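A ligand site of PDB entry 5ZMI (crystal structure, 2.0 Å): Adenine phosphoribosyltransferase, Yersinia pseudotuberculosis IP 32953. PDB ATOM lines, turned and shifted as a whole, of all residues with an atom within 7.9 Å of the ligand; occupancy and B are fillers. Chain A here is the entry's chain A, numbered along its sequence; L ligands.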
ATOM      1  N   LYS A  20      10.150  -1.378  35.879  1.00  0.00           N
ATOM      2  CA  LYS A  20       9.179  -1.295  36.947  1.00  0.00           C
ATOM      3  C   LYS A  20       7.767  -1.346  36.400  1.00  0.00           C
ATOM      4  O   LYS A  20       7.527  -0.978  35.264  1.00  0.00           O
ATOM      5  CB  LYS A  20       9.358   0.002  37.750  1.00  0.00           C
ATOM      6  CG  LYS A  20      10.515  -0.015  38.719  1.00  0.00           C
ATOM      7  CD  LYS A  20      10.702   1.378  39.321  1.00  0.00           C
ATOM      8  CE  LYS A  20      11.184   1.331  40.774  1.00  0.00           C
ATOM      9  NZ  LYS A  20      12.189   0.258  40.998  1.00  0.00           N
ATOM     10  N   THR A  21       6.848  -1.816  37.232  1.00  0.00           N
ATOM     11  CA  THR A  21       5.437  -1.850  36.897  1.00  0.00           C
ATOM     12  C   THR A  21       4.765  -0.911  37.854  1.00  0.00           C
ATOM     13  O   THR A  21       5.011  -0.958  39.056  1.00  0.00           O
ATOM     14  CB  THR A  21       4.862  -3.250  37.085  1.00  0.00           C
ATOM     15  OG1 THR A  21       5.591  -4.176  36.272  1.00  0.00           O
ATOM     16  CG2 THR A  21       3.411  -3.293  36.685  1.00  0.00           C
ATOM     17  N   ILE A  22       3.955   0.008  37.325  1.00  0.00           N
ATOM     18  CA  ILE A  22       3.283   0.970  38.177  1.00  0.00           C
ATOM     19  C   ILE A  22       1.816   0.599  38.163  1.00  0.00           C
ATOM     20  O   ILE A  22       1.133   0.826  37.160  1.00  0.00           O
ATOM     21  CB  ILE A  22       3.465   2.421  37.680  1.00  0.00           C
ATOM     22  CG1 ILE A  22       4.915   2.679  37.249  1.00  0.00           C
ATOM     23  CG2 ILE A  22       3.052   3.422  38.762  1.00  0.00           C
ATOM     24  CD1 ILE A  22       5.976   2.187  38.217  1.00  0.00           C
ATOM     25  N   TYR A  25      -1.981   3.099  36.454  1.00  0.00           N
ATOM     26  CA  TYR A  25      -1.570   4.333  35.842  1.00  0.00           C
ATOM     27  C   TYR A  25      -1.800   4.179  34.361  1.00  0.00           C
ATOM     28  O   TYR A  25      -1.486   3.157  33.800  1.00  0.00           O
ATOM     29  CB  TYR A  25      -0.127   4.657  36.140  1.00  0.00           C
ATOM     30  CG  TYR A  25       0.338   5.886  35.430  1.00  0.00           C
ATOM     31  CD1 TYR A  25       0.793   5.822  34.149  1.00  0.00           C
ATOM     32  CD2 TYR A  25       0.306   7.107  36.038  1.00  0.00           C
ATOM     33  CE1 TYR A  25       1.206   6.943  33.491  1.00  0.00           C
ATOM     34  CE2 TYR A  25       0.728   8.223  35.380  1.00  0.00           C
ATOM     35  CZ  TYR A  25       1.176   8.127  34.101  1.00  0.00           C
ATOM     36  OH  TYR A  25       1.606   9.217  33.428  1.00  0.00           O
ATOM     37  N   PRO A  26      -2.313   5.191  33.685  1.00  0.00           N
ATOM     38  CA  PRO A  26      -2.983   6.361  34.198  1.00  0.00           C
ATOM     39  C   PRO A  26      -4.252   5.914  34.842  1.00  0.00           C
ATOM     40  O   PRO A  26      -4.413   6.062  36.056  1.00  0.00           O
ATOM     41  CB  PRO A  26      -3.327   7.143  32.935  1.00  0.00           C
ATOM     42  CG  PRO A  26      -2.577   6.495  31.843  1.00  0.00           C
ATOM     43  CD  PRO A  26      -2.440   5.073  32.243  1.00  0.00           C
ATOM     44  N   ILE A  30      -5.130  -0.806  35.158  1.00  0.00           N
ATOM     45  CA  ILE A  30      -3.988  -0.879  34.211  1.00  0.00           C
ATOM     46  C   ILE A  30      -2.625  -0.991  34.905  1.00  0.00           C
ATOM     47  O   ILE A  30      -2.327  -0.221  35.829  1.00  0.00           O
ATOM     48  CB  ILE A  30      -3.961   0.382  33.330  1.00  0.00           C
ATOM     49  CG1 ILE A  30      -5.210   0.494  32.468  1.00  0.00           C
ATOM     50  CG2 ILE A  30      -2.711   0.392  32.447  1.00  0.00           C
ATOM     51  CD1 ILE A  30      -5.254  -0.469  31.304  1.00  0.00           C
ATOM     52  N   LEU A  31      -1.787  -1.938  34.478  1.00  0.00           N
ATOM     53  CA  LEU A  31      -0.423  -2.066  35.015  1.00  0.00           C
ATOM     54  C   LEU A  31       0.567  -1.416  34.046  1.00  0.00           C
ATOM     55  O   LEU A  31       0.866  -1.981  32.994  1.00  0.00           O
ATOM     56  CB  LEU A  31      -0.060  -3.552  35.200  1.00  0.00           C
ATOM     57  CG  LEU A  31      -0.845  -4.425  36.192  1.00  0.00           C
ATOM     58  CD1 LEU A  31      -0.954  -5.866  35.687  1.00  0.00           C
ATOM     59  CD2 LEU A  31      -0.208  -4.388  37.567  1.00  0.00           C
ATOM     60  N   PHE A  32       1.069  -0.228  34.356  1.00  0.00           N
ATOM     61  CA  PHE A  32       1.960   0.489  33.429  1.00  0.00           C
ATOM     62  C   PHE A  32       3.382  -0.056  33.505  1.00  0.00           C
ATOM     63  O   PHE A  32       3.957  -0.193  34.587  1.00  0.00           O
ATOM     64  CB  PHE A  32       1.926   2.009  33.699  1.00  0.00           C
ATOM     65  CG  PHE A  32       2.533   2.840  32.589  1.00  0.00           C
ATOM     66  CD1 PHE A  32       1.777   3.221  31.481  1.00  0.00           C
ATOM     67  CD2 PHE A  32       3.866   3.240  32.656  1.00  0.00           C
ATOM     68  CE1 PHE A  32       2.330   3.979  30.466  1.00  0.00           C
ATOM     69  CE2 PHE A  32       4.427   3.993  31.641  1.00  0.00           C
ATOM     70  CZ  PHE A  32       3.662   4.358  30.541  1.00  0.00           C
ATOM     71  N   ARG A  33       3.957  -0.372  32.342  1.00  0.00           N
ATOM     72  CA  ARG A  33       5.337  -0.868  32.290  1.00  0.00           C
ATOM     73  C   ARG A  33       6.246   0.276  31.933  1.00  0.00           C
ATOM     74  O   ARG A  33       6.176   0.832  30.842  1.00  0.00           O
ATOM     75  CB  ARG A  33       5.475  -2.018  31.294  1.00  0.00           C
ATOM     76  CG  ARG A  33       4.326  -3.009  31.323  1.00  0.00           C
ATOM     77  CD  ARG A  33       4.207  -3.808  32.613  1.00  0.00           C
ATOM     78  NE  ARG A  33       3.014  -4.658  32.569  1.00  0.00           N
ATOM     79  CZ  ARG A  33       2.754  -5.681  33.374  1.00  0.00           C
ATOM     80  NH1 ARG A  33       1.624  -6.363  33.210  1.00  0.00           N
ATOM     81  NH2 ARG A  33       3.605  -6.016  34.333  1.00  0.00           N
ATOM     82  N   ASP A  34       7.099   0.630  32.880  1.00  0.00           N
ATOM     83  CA  ASP A  34       7.842   1.879  32.840  1.00  0.00           C
ATOM     84  C   ASP A  34       9.282   1.627  32.488  1.00  0.00           C
ATOM     85  O   ASP A  34      10.028   1.139  33.321  1.00  0.00           O
ATOM     86  CB  ASP A  34       7.718   2.555  34.191  1.00  0.00           C
ATOM     87  CG  ASP A  34       8.655   3.771  34.389  1.00  0.00           C
ATOM     88  OD1 ASP A  34       9.209   4.355  33.405  1.00  0.00           O
ATOM     89  OD2 ASP A  34       8.819   4.154  35.595  1.00  0.00           O
ATOM     90  N   VAL A  35       9.679   2.030  31.289  1.00  0.00           N
ATOM     91  CA  VAL A  35      11.035   1.818  30.845  1.00  0.00           C
ATOM     92  C   VAL A  35      12.046   2.798  31.363  1.00  0.00           C
ATOM     93  O   VAL A  35      13.228   2.621  31.109  1.00  0.00           O
ATOM     94  CB  VAL A  35      11.183   1.849  29.317  1.00  0.00           C
ATOM     95  CG1 VAL A  35      10.356   0.769  28.716  1.00  0.00           C
ATOM     96  CG2 VAL A  35      10.811   3.194  28.716  1.00  0.00           C
ATOM     97  N   ARG A  70      10.038   8.286  22.567  1.00  0.00           N
ATOM     98  CA  ARG A  70      10.587   7.175  23.314  1.00  0.00           C
ATOM     99  C   ARG A  70      11.193   6.162  22.410  1.00  0.00           C
ATOM    100  O   ARG A  70      12.091   5.414  22.802  1.00  0.00           O
ATOM    101  CB  ARG A  70       9.485   6.574  24.150  1.00  0.00           C
ATOM    102  CG  ARG A  70       9.040   7.580  25.204  1.00  0.00           C
ATOM    103  CD  ARG A  70       9.316   7.089  26.616  1.00  0.00           C
ATOM    104  NE  ARG A  70       8.588   5.843  26.805  1.00  0.00           N
ATOM    105  CZ  ARG A  70       7.262   5.742  26.964  1.00  0.00           C
ATOM    106  NH1 ARG A  70       6.706   4.532  27.100  1.00  0.00           N
ATOM    107  NH2 ARG A  70       6.497   6.822  27.009  1.00  0.00           N
ATOM    108  N   ASP A 131      10.120   1.563  21.811  1.00  0.00           N
ATOM    109  CA  ASP A 131      10.292   1.035  23.152  1.00  0.00           C
ATOM    110  C   ASP A 131       9.299  -0.093  23.468  1.00  0.00           C
ATOM    111  O   ASP A 131       9.657  -1.128  24.068  1.00  0.00           O
ATOM    112  CB  ASP A 131      10.229   2.193  24.226  1.00  0.00           C
ATOM    113  CG  ASP A 131       8.903   2.958  24.222  1.00  0.00           C
ATOM    114  OD1 ASP A 131       8.145   2.901  23.220  1.00  0.00           O
ATOM    115  OD2 ASP A 131       8.629   3.625  25.230  1.00  0.00           O
ATOM    116  N   LEU A 132       8.048   0.083  23.084  1.00  0.00           N
ATOM    117  CA  LEU A 132       6.992  -0.782  23.548  1.00  0.00           C
ATOM    118  C   LEU A 132       5.974  -0.958  22.432  1.00  0.00           C
ATOM    119  O   LEU A 132       5.660  -0.003  21.753  1.00  0.00           O
ATOM    120  CB  LEU A 132       6.346  -0.178  24.774  1.00  0.00           C
ATOM    121  CG  LEU A 132       5.256  -0.952  25.507  1.00  0.00           C
ATOM    122  CD1 LEU A 132       5.326  -0.714  26.994  1.00  0.00           C
ATOM    123  CD2 LEU A 132       3.901  -0.535  24.950  1.00  0.00           C
ATOM    124  N   LEU A 133       5.489  -2.177  22.206  1.00  0.00           N
ATOM    125  CA  LEU A 133       4.439  -2.432  21.224  1.00  0.00           C
ATOM    126  C   LEU A 133       3.134  -2.666  21.973  1.00  0.00           C
ATOM    127  O   LEU A 133       2.986  -3.639  22.733  1.00  0.00           O
ATOM    128  CB  LEU A 133       4.769  -3.653  20.362  1.00  0.00           C
ATOM    129  CG  LEU A 133       3.754  -4.041  19.280  1.00  0.00           C
ATOM    130  CD1 LEU A 133       3.537  -2.894  18.290  1.00  0.00           C
ATOM    131  CD2 LEU A 133       4.157  -5.319  18.542  1.00  0.00           C
ATOM    132  N   ALA A 134       2.176  -1.787  21.722  1.00  0.00           N
ATOM    133  CA  ALA A 134       0.890  -1.890  22.352  1.00  0.00           C
ATOM    134  C   ALA A 134      -0.087  -2.194  21.231  1.00  0.00           C
ATOM    135  O   ALA A 134      -0.169  -3.335  20.751  1.00  0.00           O
ATOM    136  CB  ALA A 134       0.569  -0.572  23.090  1.00  0.00           C
ATOM    137  N   THR A 135      -0.789  -1.191  20.744  1.00  0.00           N
ATOM    138  CA  THR A 135      -1.779  -1.419  19.684  1.00  0.00           C
ATOM    139  C   THR A 135      -1.153  -1.506  18.306  1.00  0.00           C
ATOM    140  O   THR A 135      -1.698  -2.146  17.425  1.00  0.00           O
ATOM    141  CB  THR A 135      -2.848  -0.302  19.699  1.00  0.00           C
ATOM    142  OG1 THR A 135      -2.248   0.931  19.284  1.00  0.00           O
ATOM    143  CG2 THR A 135      -3.433  -0.127  21.101  1.00  0.00           C
ATOM    144  N   ILE A 160       9.658  -3.998  24.822  1.00  0.00           N
ATOM    145  CA  ILE A 160       8.522  -4.594  25.478  1.00  0.00           C
ATOM    146  C   ILE A 160       7.393  -4.862  24.477  1.00  0.00           C
ATOM    147  O   ILE A 160       7.022  -3.980  23.685  1.00  0.00           O
ATOM    148  CB  ILE A 160       7.946  -3.673  26.562  1.00  0.00           C
ATOM    149  CG1 ILE A 160       9.009  -3.321  27.603  1.00  0.00           C
ATOM    150  CG2 ILE A 160       6.776  -4.344  27.253  1.00  0.00           C
ATOM    151  CD1 ILE A 160       8.514  -2.341  28.646  1.00  0.00           C
ATOM    152  N   LEU A 162       3.383  -6.044  24.500  1.00  0.00           N
ATOM    153  CA  LEU A 162       2.165  -6.311  25.262  1.00  0.00           C
ATOM    154  C   LEU A 162       1.188  -6.949  24.306  1.00  0.00           C
ATOM    155  O   LEU A 162       0.324  -6.258  23.764  1.00  0.00           O
ATOM    156  CB  LEU A 162       1.540  -5.028  25.800  1.00  0.00           C
ATOM    157  CG  LEU A 162       2.485  -4.186  26.646  1.00  0.00           C
ATOM    158  CD1 LEU A 162       1.782  -2.935  27.104  1.00  0.00           C
ATOM    159  CD2 LEU A 162       3.021  -4.977  27.813  1.00  0.00           C
ATOM    160  N   GLU A 164      -1.507  -8.795  24.245  1.00  0.00           N
ATOM    161  CA  GLU A 164      -2.955  -8.807  24.389  1.00  0.00           C
ATOM    162  C   GLU A 164      -3.595  -7.523  23.830  1.00  0.00           C
ATOM    163  O   GLU A 164      -4.800  -7.487  23.573  1.00  0.00           O
ATOM    164  CB  GLU A 164      -3.343  -9.066  25.860  1.00  0.00           C
ATOM    165  CG  GLU A 164      -3.473  -7.841  26.762  1.00  0.00           C
ATOM    166  CD  GLU A 164      -2.149  -7.272  27.281  1.00  0.00           C
ATOM    167  OE1 GLU A 164      -1.053  -7.789  26.932  1.00  0.00           O
ATOM    168  OE2 GLU A 164      -2.228  -6.290  28.063  1.00  0.00           O
ATOM    169  N   LEU A 165      -2.807  -6.468  23.631  1.00  0.00           N
ATOM    170  CA  LEU A 165      -3.335  -5.248  23.025  1.00  0.00           C
ATOM    171  C   LEU A 165      -3.355  -5.342  21.506  1.00  0.00           C
ATOM    172  O   LEU A 165      -3.786  -4.407  20.850  1.00  0.00           O
ATOM    173  CB  LEU A 165      -2.550  -4.020  23.495  1.00  0.00           C
ATOM    174  CG  LEU A 165      -2.856  -3.670  24.942  1.00  0.00           C
ATOM    175  CD1 LEU A 165      -2.042  -2.453  25.398  1.00  0.00           C
ATOM    176  CD2 LEU A 165      -4.351  -3.469  25.128  1.00  0.00           C
ATOM    177  N   PHE A 184       4.665  -8.705  28.607  1.00  0.00           N
ATOM    178  CA  PHE A 184       3.819  -8.689  29.790  1.00  0.00           C
ATOM    179  C   PHE A 184       2.346  -8.709  29.333  1.00  0.00           C
ATOM    180  O   PHE A 184       2.031  -8.445  28.155  1.00  0.00           O
ATOM    181  CB  PHE A 184       3.980  -7.404  30.623  1.00  0.00           C
ATOM    182  CG  PHE A 184       5.379  -7.081  31.117  1.00  0.00           C
ATOM    183  CD1 PHE A 184       5.810  -7.502  32.370  1.00  0.00           C
ATOM    184  CD2 PHE A 184       6.209  -6.216  30.390  1.00  0.00           C
ATOM    185  CE1 PHE A 184       7.055  -7.144  32.854  1.00  0.00           C
ATOM    186  CE2 PHE A 184       7.454  -5.858  30.874  1.00  0.00           C
ATOM    187  CZ  PHE A 184       7.882  -6.323  32.111  1.00  0.00           C
ATOM    188  N   ASP A 185       1.442  -8.940  30.281  1.00  0.00           N
ATOM    189  CA  ASP A 185       0.012  -8.736  30.071  1.00  0.00           C
ATOM    190  C   ASP A 185      -0.487  -7.744  31.110  1.00  0.00           C
ATOM    191  O   ASP A 185      -1.671  -7.726  31.444  1.00  0.00           O
ATOM    192  CB  ASP A 185      -0.732 -10.086  30.160  1.00  0.00           C
ATOM    193  CG  ASP A 185       0.147 -11.257  29.740  1.00  0.00           C
ATOM    194  OD1 ASP A 185       0.612 -11.288  28.586  1.00  0.00           O
ATOM    195  OD2 ASP A 185       0.380 -12.139  30.596  1.00  0.00           O
HETATM  196  N1  LIG L   1       0.524   1.576  26.435  1.00  0.00           N
HETATM  197  C1  LIG L   1      -0.680   0.921  26.464  1.00  0.00           C
HETATM  198  N2  LIG L   1      -0.742   0.125  27.575  1.00  0.00           N
HETATM  199  C2  LIG L   1       0.437   0.271  28.240  1.00  0.00           C
HETATM  200  C3  LIG L   1       1.053  -0.270  29.471  1.00  0.00           C
HETATM  201  N3  LIG L   1       0.353  -1.152  30.217  1.00  0.00           N
HETATM  202  N4  LIG L   1       2.310   0.131  29.828  1.00  0.00           N
HETATM  203  C4  LIG L   1       3.008   1.009  29.094  1.00  0.00           C
HETATM  204  N5  LIG L   1       2.497   1.527  27.967  1.00  0.00           N
HETATM  205  C5  LIG L   1       1.261   1.204  27.489  1.00  0.00           C
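A nitrogen (N3) of the ligand lies within hydrogen-bond range of the backbone carbonyl oxygen (O) of Leu 31, 2.9 Å away. A nitrogen (N4) of the ligand lies within hydrogen-bond range of the backbone NH of Arg 33 (3.0 Å).
N of Leu 162 is in hydrogen-bond range of O of Leu 133 (3.0 Å). The backbone carbonyl oxygen (O) of Leu 31 is in hydrogen-bond range of the guanidinium group (NE) of Arg 33, at 3.5 Å. NH2 of Arg 33 is in hydrogen-bond range of OG1 of Thr 21 (3.3 Å). The backbone carbonyl oxygen (O) of Phe 32 sits at hydrogen-bond distance from the backbone NH (N) of Ile 22 (2.7 Å).
Merely in contact with the ligand: Phe 32, Leu 132, Leu 165, Leu 162 and Ala 134.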
